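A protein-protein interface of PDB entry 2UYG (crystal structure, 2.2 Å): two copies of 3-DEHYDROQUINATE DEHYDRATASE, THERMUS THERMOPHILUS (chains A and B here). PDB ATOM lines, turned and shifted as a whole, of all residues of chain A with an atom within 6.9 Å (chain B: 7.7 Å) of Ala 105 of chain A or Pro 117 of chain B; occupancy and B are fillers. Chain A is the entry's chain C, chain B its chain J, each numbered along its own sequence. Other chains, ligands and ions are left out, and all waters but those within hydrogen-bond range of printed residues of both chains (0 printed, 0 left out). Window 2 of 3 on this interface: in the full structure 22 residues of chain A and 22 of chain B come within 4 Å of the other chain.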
ATOM      1  N   ASN A 102       0.651  -7.368   1.343  1.00  0.00           N
ATOM      2  CA  ASN A 102       0.518  -8.185   0.167  1.00  0.00           C
ATOM      3  C   ASN A 102       1.838  -8.166  -0.517  1.00  0.00           C
ATOM      4  O   ASN A 102       2.135  -7.187  -1.148  1.00  0.00           O
ATOM      5  CB  ASN A 102      -0.536  -7.591  -0.777  1.00  0.00           C
ATOM      6  CG  ASN A 102      -0.862  -8.496  -1.943  1.00  0.00           C
ATOM      7  OD1 ASN A 102      -0.114  -9.416  -2.290  1.00  0.00           O
ATOM      8  ND2 ASN A 102      -1.989  -8.229  -2.576  1.00  0.00           N
ATOM      9  N   LEU A 103       2.593  -9.247  -0.463  1.00  0.00           N
ATOM     10  CA  LEU A 103       3.889  -9.311  -1.170  1.00  0.00           C
ATOM     11  C   LEU A 103       3.804  -9.100  -2.685  1.00  0.00           C
ATOM     12  O   LEU A 103       4.786  -8.704  -3.295  1.00  0.00           O
ATOM     13  CB  LEU A 103       4.575 -10.633  -0.929  1.00  0.00           C
ATOM     14  CG  LEU A 103       4.754 -11.062   0.528  1.00  0.00           C
ATOM     15  CD1 LEU A 103       5.270 -12.414   0.587  1.00  0.00           C
ATOM     16  CD2 LEU A 103       5.726 -10.194   1.226  1.00  0.00           C
ATOM     17  N   HIS A 104       2.641  -9.306  -3.300  1.00  0.00           N
ATOM     18  CA  HIS A 104       2.497  -9.165  -4.742  1.00  0.00           C
ATOM     19  C   HIS A 104       2.174  -7.749  -5.253  1.00  0.00           C
ATOM     20  O   HIS A 104       1.972  -7.575  -6.437  1.00  0.00           O
ATOM     21  CB  HIS A 104       1.480 -10.197  -5.232  1.00  0.00           C
ATOM     22  CG  HIS A 104       1.823 -11.589  -4.799  1.00  0.00           C
ATOM     23  ND1 HIS A 104       1.105 -12.257  -3.845  1.00  0.00           N
ATOM     24  CD2 HIS A 104       2.883 -12.383  -5.084  1.00  0.00           C
ATOM     25  CE1 HIS A 104       1.635 -13.452  -3.638  1.00  0.00           C
ATOM     26  NE2 HIS A 104       2.736 -13.538  -4.358  1.00  0.00           N
ATOM     27  N   ALA A 105       2.099  -6.763  -4.368  1.00  0.00           N
ATOM     28  CA  ALA A 105       1.845  -5.386  -4.762  1.00  0.00           C
ATOM     29  C   ALA A 105       3.000  -4.442  -4.382  1.00  0.00           C
ATOM     30  O   ALA A 105       2.814  -3.222  -4.307  1.00  0.00           O
ATOM     31  CB  ALA A 105       0.548  -4.880  -4.090  1.00  0.00           C
ATOM     32  N   ARG A 106       4.157  -5.029  -4.089  1.00  0.00           N
ATOM     33  CA  ARG A 106       5.399  -4.313  -3.797  1.00  0.00           C
ATOM     34  C   ARG A 106       6.522  -4.791  -4.782  1.00  0.00           C
ATOM     35  O   ARG A 106       6.249  -5.209  -5.901  1.00  0.00           O
ATOM     36  CB  ARG A 106       5.753  -4.462  -2.306  1.00  0.00           C
ATOM     37  CG  ARG A 106       4.525  -4.295  -1.310  1.00  0.00           C
ATOM     38  CD  ARG A 106       4.812  -4.588   0.230  1.00  0.00           C
ATOM     39  NE  ARG A 106       6.075  -4.018   0.695  1.00  0.00           N
ATOM     40  CZ  ARG A 106       6.666  -4.287   1.866  1.00  0.00           C
ATOM     41  NH1 ARG A 106       7.858  -3.712   2.145  1.00  0.00           N
ATOM     42  NH2 ARG A 106       6.057  -5.058   2.781  1.00  0.00           N
ATOM     43  N   GLU A 107       7.775  -4.782  -4.333  1.00  0.00           N
ATOM     44  CA  GLU A 107       8.928  -4.896  -5.239  1.00  0.00           C
ATOM     45  C   GLU A 107       8.904  -6.277  -5.726  1.00  0.00           C
ATOM     46  O   GLU A 107       8.375  -7.116  -5.050  1.00  0.00           O
ATOM     47  CB  GLU A 107      10.279  -4.622  -4.521  1.00  0.00           C
ATOM     48  CG  GLU A 107      10.393  -3.249  -3.840  1.00  0.00           C
ATOM     49  CD  GLU A 107       9.844  -3.204  -2.420  1.00  0.00           C
ATOM     50  OE1 GLU A 107       8.811  -3.822  -2.162  1.00  0.00           O
ATOM     51  OE2 GLU A 107      10.414  -2.514  -1.531  1.00  0.00           O
ATOM     52  N   ARG A 111       8.049 -11.083  -4.025  1.00  0.00           N
ATOM     53  CA  ARG A 111       7.049 -11.966  -4.559  1.00  0.00           C
ATOM     54  C   ARG A 111       7.445 -13.408  -4.458  1.00  0.00           C
ATOM     55  O   ARG A 111       6.610 -14.256  -4.651  1.00  0.00           O
ATOM     56  CB  ARG A 111       6.760 -11.594  -6.033  1.00  0.00           C
ATOM     57  CG  ARG A 111       6.179 -10.193  -6.175  1.00  0.00           C
ATOM     58  CD  ARG A 111       5.518  -9.842  -7.518  1.00  0.00           C
ATOM     59  NE  ARG A 111       4.310 -10.658  -7.639  1.00  0.00           N
ATOM     60  CZ  ARG A 111       3.515 -10.675  -8.667  1.00  0.00           C
ATOM     61  NH1 ARG A 111       3.757  -9.876  -9.697  1.00  0.00           N
ATOM     62  NH2 ARG A 111       2.466 -11.505  -8.647  1.00  0.00           N
ATOM     63  N   THR B  78      -5.569 -17.821 -12.511  1.00  0.00           N
ATOM     64  CA  THR B  78      -4.697 -16.996 -11.704  1.00  0.00           C
ATOM     65  C   THR B  78      -3.291 -16.853 -12.223  1.00  0.00           C
ATOM     66  O   THR B  78      -2.666 -15.886 -11.931  1.00  0.00           O
ATOM     67  CB  THR B  78      -4.725 -17.361 -10.140  1.00  0.00           C
ATOM     68  OG1 THR B  78      -3.441 -17.743  -9.603  1.00  0.00           O
ATOM     69  CG2 THR B  78      -5.675 -18.435  -9.757  1.00  0.00           C
ATOM     70  N   TYR B  82      -4.726 -11.701 -17.389  1.00  0.00           N
ATOM     71  CA  TYR B  82      -4.549 -10.293 -17.081  1.00  0.00           C
ATOM     72  C   TYR B  82      -5.848  -9.516 -17.303  1.00  0.00           C
ATOM     73  O   TYR B  82      -5.949  -8.376 -16.854  1.00  0.00           O
ATOM     74  CB  TYR B  82      -3.369  -9.644 -17.899  1.00  0.00           C
ATOM     75  CG  TYR B  82      -1.922 -10.134 -17.574  1.00  0.00           C
ATOM     76  CD1 TYR B  82      -1.218 -11.041 -18.428  1.00  0.00           C
ATOM     77  CD2 TYR B  82      -1.242  -9.634 -16.468  1.00  0.00           C
ATOM     78  CE1 TYR B  82       0.083 -11.420 -18.156  1.00  0.00           C
ATOM     79  CE2 TYR B  82       0.040 -10.019 -16.160  1.00  0.00           C
ATOM     80  CZ  TYR B  82       0.710 -10.890 -16.983  1.00  0.00           C
ATOM     81  OH  TYR B  82       2.014 -11.180 -16.626  1.00  0.00           O
ATOM     82  N   LEU B  85      -7.403  -9.496 -14.009  1.00  0.00           N
ATOM     83  CA  LEU B  85      -6.697  -8.534 -13.154  1.00  0.00           C
ATOM     84  C   LEU B  85      -7.291  -7.158 -13.383  1.00  0.00           C
ATOM     85  O   LEU B  85      -7.510  -6.376 -12.472  1.00  0.00           O
ATOM     86  CB  LEU B  85      -5.221  -8.505 -13.568  1.00  0.00           C
ATOM     87  CG  LEU B  85      -4.081  -7.820 -12.791  1.00  0.00           C
ATOM     88  CD1 LEU B  85      -3.237  -6.950 -13.729  1.00  0.00           C
ATOM     89  CD2 LEU B  85      -4.406  -7.137 -11.497  1.00  0.00           C
ATOM     90  N   ILE B  88     -10.763  -6.889 -11.754  1.00  0.00           N
ATOM     91  CA  ILE B  88     -10.721  -6.564 -10.334  1.00  0.00           C
ATOM     92  C   ILE B  88     -10.300  -5.124 -10.066  1.00  0.00           C
ATOM     93  O   ILE B  88     -10.874  -4.506  -9.178  1.00  0.00           O
ATOM     94  CB  ILE B  88      -9.996  -7.554  -9.393  1.00  0.00           C
ATOM     95  CG1 ILE B  88      -8.804  -6.887  -8.810  1.00  0.00           C
ATOM     96  CG2 ILE B  88      -9.689  -8.929  -9.913  1.00  0.00           C
ATOM     97  CD1 ILE B  88      -9.117  -6.461  -7.429  1.00  0.00           C
ATOM     98  N   ARG B  89      -9.371  -4.588 -10.871  1.00  0.00           N
ATOM     99  CA  ARG B  89      -8.903  -3.196 -10.719  1.00  0.00           C
ATOM    100  C   ARG B  89      -9.990  -2.199 -11.141  1.00  0.00           C
ATOM    101  O   ARG B  89     -10.035  -1.070 -10.650  1.00  0.00           O
ATOM    102  CB  ARG B  89      -7.610  -2.861 -11.548  1.00  0.00           C
ATOM    103  CG  ARG B  89      -6.228  -3.457 -11.104  1.00  0.00           C
ATOM    104  CD  ARG B  89      -5.334  -2.494 -10.250  1.00  0.00           C
ATOM    105  NE  ARG B  89      -6.075  -1.975  -9.064  1.00  0.00           N
ATOM    106  CZ  ARG B  89      -6.813  -0.834  -9.029  1.00  0.00           C
ATOM    107  NH1 ARG B  89      -7.449  -0.500  -7.904  1.00  0.00           N
ATOM    108  NH2 ARG B  89      -6.920  -0.011 -10.079  1.00  0.00           N
ATOM    109  N   GLU B  97      -8.054 -13.059  -2.639  1.00  0.00           N
ATOM    110  CA  GLU B  97      -7.764 -14.244  -3.422  1.00  0.00           C
ATOM    111  C   GLU B  97      -7.583 -15.429  -2.508  1.00  0.00           C
ATOM    112  O   GLU B  97      -6.903 -15.313  -1.533  1.00  0.00           O
ATOM    113  CB  GLU B  97      -6.487 -14.050  -4.226  1.00  0.00           C
ATOM    114  CG  GLU B  97      -6.341 -15.047  -5.337  1.00  0.00           C
ATOM    115  CD  GLU B  97      -5.118 -14.782  -6.180  1.00  0.00           C
ATOM    116  OE1 GLU B  97      -4.285 -15.749  -6.275  1.00  0.00           O
ATOM    117  OE2 GLU B  97      -4.977 -13.630  -6.686  1.00  0.00           O
ATOM    118  N   HIS B 112       3.185 -18.155  -9.652  1.00  0.00           N
ATOM    119  CA  HIS B 112       3.013 -16.729  -9.897  1.00  0.00           C
ATOM    120  C   HIS B 112       1.506 -16.426 -10.143  1.00  0.00           C
ATOM    121  O   HIS B 112       0.835 -17.165 -10.842  1.00  0.00           O
ATOM    122  CB  HIS B 112       4.060 -16.266 -10.943  1.00  0.00           C
ATOM    123  CG  HIS B 112       3.569 -16.111 -12.333  1.00  0.00           C
ATOM    124  ND1 HIS B 112       2.592 -16.912 -12.898  1.00  0.00           N
ATOM    125  CD2 HIS B 112       3.970 -15.256 -13.320  1.00  0.00           C
ATOM    126  CE1 HIS B 112       2.398 -16.553 -14.162  1.00  0.00           C
ATOM    127  NE2 HIS B 112       3.225 -15.553 -14.447  1.00  0.00           N
ATOM    128  N   SER B 113       0.947 -15.446  -9.451  1.00  0.00           N
ATOM    129  CA  SER B 113      -0.448 -15.055  -9.649  1.00  0.00           C
ATOM    130  C   SER B 113      -0.497 -13.679 -10.165  1.00  0.00           C
ATOM    131  O   SER B 113      -0.010 -12.779  -9.502  1.00  0.00           O
ATOM    132  CB  SER B 113      -1.241 -15.042  -8.367  1.00  0.00           C
ATOM    133  OG  SER B 113      -2.367 -14.202  -8.521  1.00  0.00           O
ATOM    134  N   VAL B 114      -1.078 -13.506 -11.346  1.00  0.00           N
ATOM    135  CA  VAL B 114      -1.208 -12.177 -11.928  1.00  0.00           C
ATOM    136  C   VAL B 114      -2.396 -11.412 -11.319  1.00  0.00           C
ATOM    137  O   VAL B 114      -2.512 -10.262 -11.559  1.00  0.00           O
ATOM    138  CB  VAL B 114      -1.360 -12.236 -13.476  1.00  0.00           C
ATOM    139  CG1 VAL B 114      -0.173 -12.938 -14.185  1.00  0.00           C
ATOM    140  CG2 VAL B 114      -2.580 -12.940 -13.875  1.00  0.00           C
ATOM    141  N   THR B 115      -3.277 -12.049 -10.533  1.00  0.00           N
ATOM    142  CA  THR B 115      -4.428 -11.344  -9.932  1.00  0.00           C
ATOM    143  C   THR B 115      -4.085 -10.776  -8.572  1.00  0.00           C
ATOM    144  O   THR B 115      -4.538  -9.678  -8.202  1.00  0.00           O
ATOM    145  CB  THR B 115      -5.692 -12.234  -9.836  1.00  0.00           C
ATOM    146  OG1 THR B 115      -5.354 -13.552  -9.392  1.00  0.00           O
ATOM    147  CG2 THR B 115      -6.263 -12.456 -11.261  1.00  0.00           C
ATOM    148  N   ALA B 116      -3.227 -11.501  -7.866  1.00  0.00           N
ATOM    149  CA  ALA B 116      -2.766 -11.112  -6.546  1.00  0.00           C
ATOM    150  C   ALA B 116      -2.389  -9.622  -6.320  1.00  0.00           C
ATOM    151  O   ALA B 116      -2.717  -9.031  -5.261  1.00  0.00           O
ATOM    152  CB  ALA B 116      -1.581 -12.091  -6.101  1.00  0.00           C
ATOM    153  N   PRO B 117      -1.689  -8.972  -7.262  1.00  0.00           N
ATOM    154  CA  PRO B 117      -1.315  -7.544  -7.033  1.00  0.00           C
ATOM    155  C   PRO B 117      -2.461  -6.502  -6.785  1.00  0.00           C
ATOM    156  O   PRO B 117      -2.221  -5.381  -6.322  1.00  0.00           O
ATOM    157  CB  PRO B 117      -0.572  -7.189  -8.299  1.00  0.00           C
ATOM    158  CG  PRO B 117      -0.022  -8.446  -8.770  1.00  0.00           C
ATOM    159  CD  PRO B 117      -1.101  -9.493  -8.519  1.00  0.00           C
ATOM    160  N   ALA B 118      -3.679  -6.872  -7.170  1.00  0.00           N
ATOM    161  CA  ALA B 118      -4.851  -6.016  -7.120  1.00  0.00           C
ATOM    162  C   ALA B 118      -5.817  -6.427  -6.015  1.00  0.00           C
ATOM    163  O   ALA B 118      -6.796  -5.750  -5.784  1.00  0.00           O
ATOM    164  CB  ALA B 118      -5.559  -6.062  -8.461  1.00  0.00           C
ATOM    165  N   CYS B 119      -5.495  -7.491  -5.321  1.00  0.00           N
ATOM    166  CA  CYS B 119      -6.233  -7.983  -4.176  1.00  0.00           C
ATOM    167  C   CYS B 119      -5.763  -7.409  -2.889  1.00  0.00           C
ATOM    168  O   CYS B 119      -4.568  -7.034  -2.728  1.00  0.00           O
ATOM    169  CB  CYS B 119      -6.088  -9.511  -4.110  1.00  0.00           C
ATOM    170  SG  CYS B 119      -6.940 -10.271  -5.569  1.00  0.00           S
ATOM    171  N   ARG B 120      -6.694  -7.360  -1.957  1.00  0.00           N
ATOM    172  CA  ARG B 120      -6.396  -6.985  -0.586  1.00  0.00           C
ATOM    173  C   ARG B 120      -5.347  -7.923  -0.055  1.00  0.00           C
ATOM    174  O   ARG B 120      -4.413  -7.492   0.597  1.00  0.00           O
ATOM    175  CB  ARG B 120      -7.590  -7.231   0.308  1.00  0.00           C
ATOM    176  CG  ARG B 120      -8.282  -6.099   0.906  1.00  0.00           C
ATOM    177  CD  ARG B 120      -7.515  -4.875   1.519  1.00  0.00           C
ATOM    178  NE  ARG B 120      -8.286  -3.832   0.834  1.00  0.00           N
ATOM    179  CZ  ARG B 120      -9.254  -3.048   1.309  1.00  0.00           C
ATOM    180  NH1 ARG B 120      -9.880  -2.216   0.465  1.00  0.00           N
ATOM    181  NH2 ARG B 120      -9.570  -3.012   2.596  1.00  0.00           N
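Printed residues of chain B within 4 Å of Asn 102 of chain A: Ala 116 and Cys 119. Printed residues of chain B within 4 Å of Arg 111 of chain A: Ser 113 (2.9 Å) and Pro 117 (3.9 Å). Pro 117 of chain B touches just these residues of chain A: His 104 (3.2 Å), Ala 105 (3.6 Å) and Arg 111 (3.9 Å). Of the printed residues of chain A, Cys 119 of chain B touches Asn 102. The nearest residue of chain A that does not touch Pro 117 of chain B is Asn 102 of chain A (4.6 Å). The nearest printed residue of chain B that does not touch His 104 of chain A is Ser 113 of chain B (5.2 Å).
Among the printed residues, pairs that only touch across the chains: His 104 of chain A with Ala 116 of chain B, His 104 of chain A with Pro 117 of chain B, Ala 105 of chain A with Pro 117 of chain B and Arg 111 of chain A with Pro 117 of chain B.
ND2 of Asn 102 of chain A lies within hydrogen-bond range of O of Cys 119 of chain B. The backbone carbonyl oxygen (O) of Ser 113 of chain B sits at hydrogen-bond distance from the guanidinium group (NH2) of Arg 111 of chain A (2.9 Å). The backbone carbonyl oxygen (O) of Ala 116 of chain B lies within hydrogen-bond range of the side-chain amide nitrogen (ND2) of Asn 102 of chain A (2.9 Å).
No position is printed for both chains.
OE2 of Glu 97 of chain B lies within hydrogen-bond range of N of Ala 116 of chain B (3.0 Å). SG of Cys 119 of chain B sits at hydrogen-bond distance from O of Thr 115 of chain B, at 3.6 Å. OG of Ser 113 of chain B is in hydrogen-bond range of N of Ala 116 of chain B (2.9 Å). The side-chain carboxylate (OE2) of Glu 97 of chain B is in hydrogen-bond range of the side-chain hydroxyl (OG) of Ser 113 of chain B, 3.2 Å away. OD1 of Asn 102 of chain A sits at hydrogen-bond distance from N of His 104 of chain A, 2.9 Å away. OG of Ser 113 of chain B is in hydrogen-bond range of N of Thr 115 of chain B.
Of the 7 printed residues of chain A, 4 touch a printed residue of chain B. Hydrophobic or aromatic side chains of chain A within 4 Å of the printed part of chain B: His 104 and Ala 105. Of the 15 printed residues of chain B, 4 touch a printed residue of chain A. Printed residues of chain B that touch a printed residue of chain A: Ser 113, Ala 116, Pro 117 and Cys 119. Hydrophobic or aromatic side chains of chain B that line the printed part of chain A: Ala 116 and Pro 117. Among the printed residues, 7 pairs touch across the chains.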
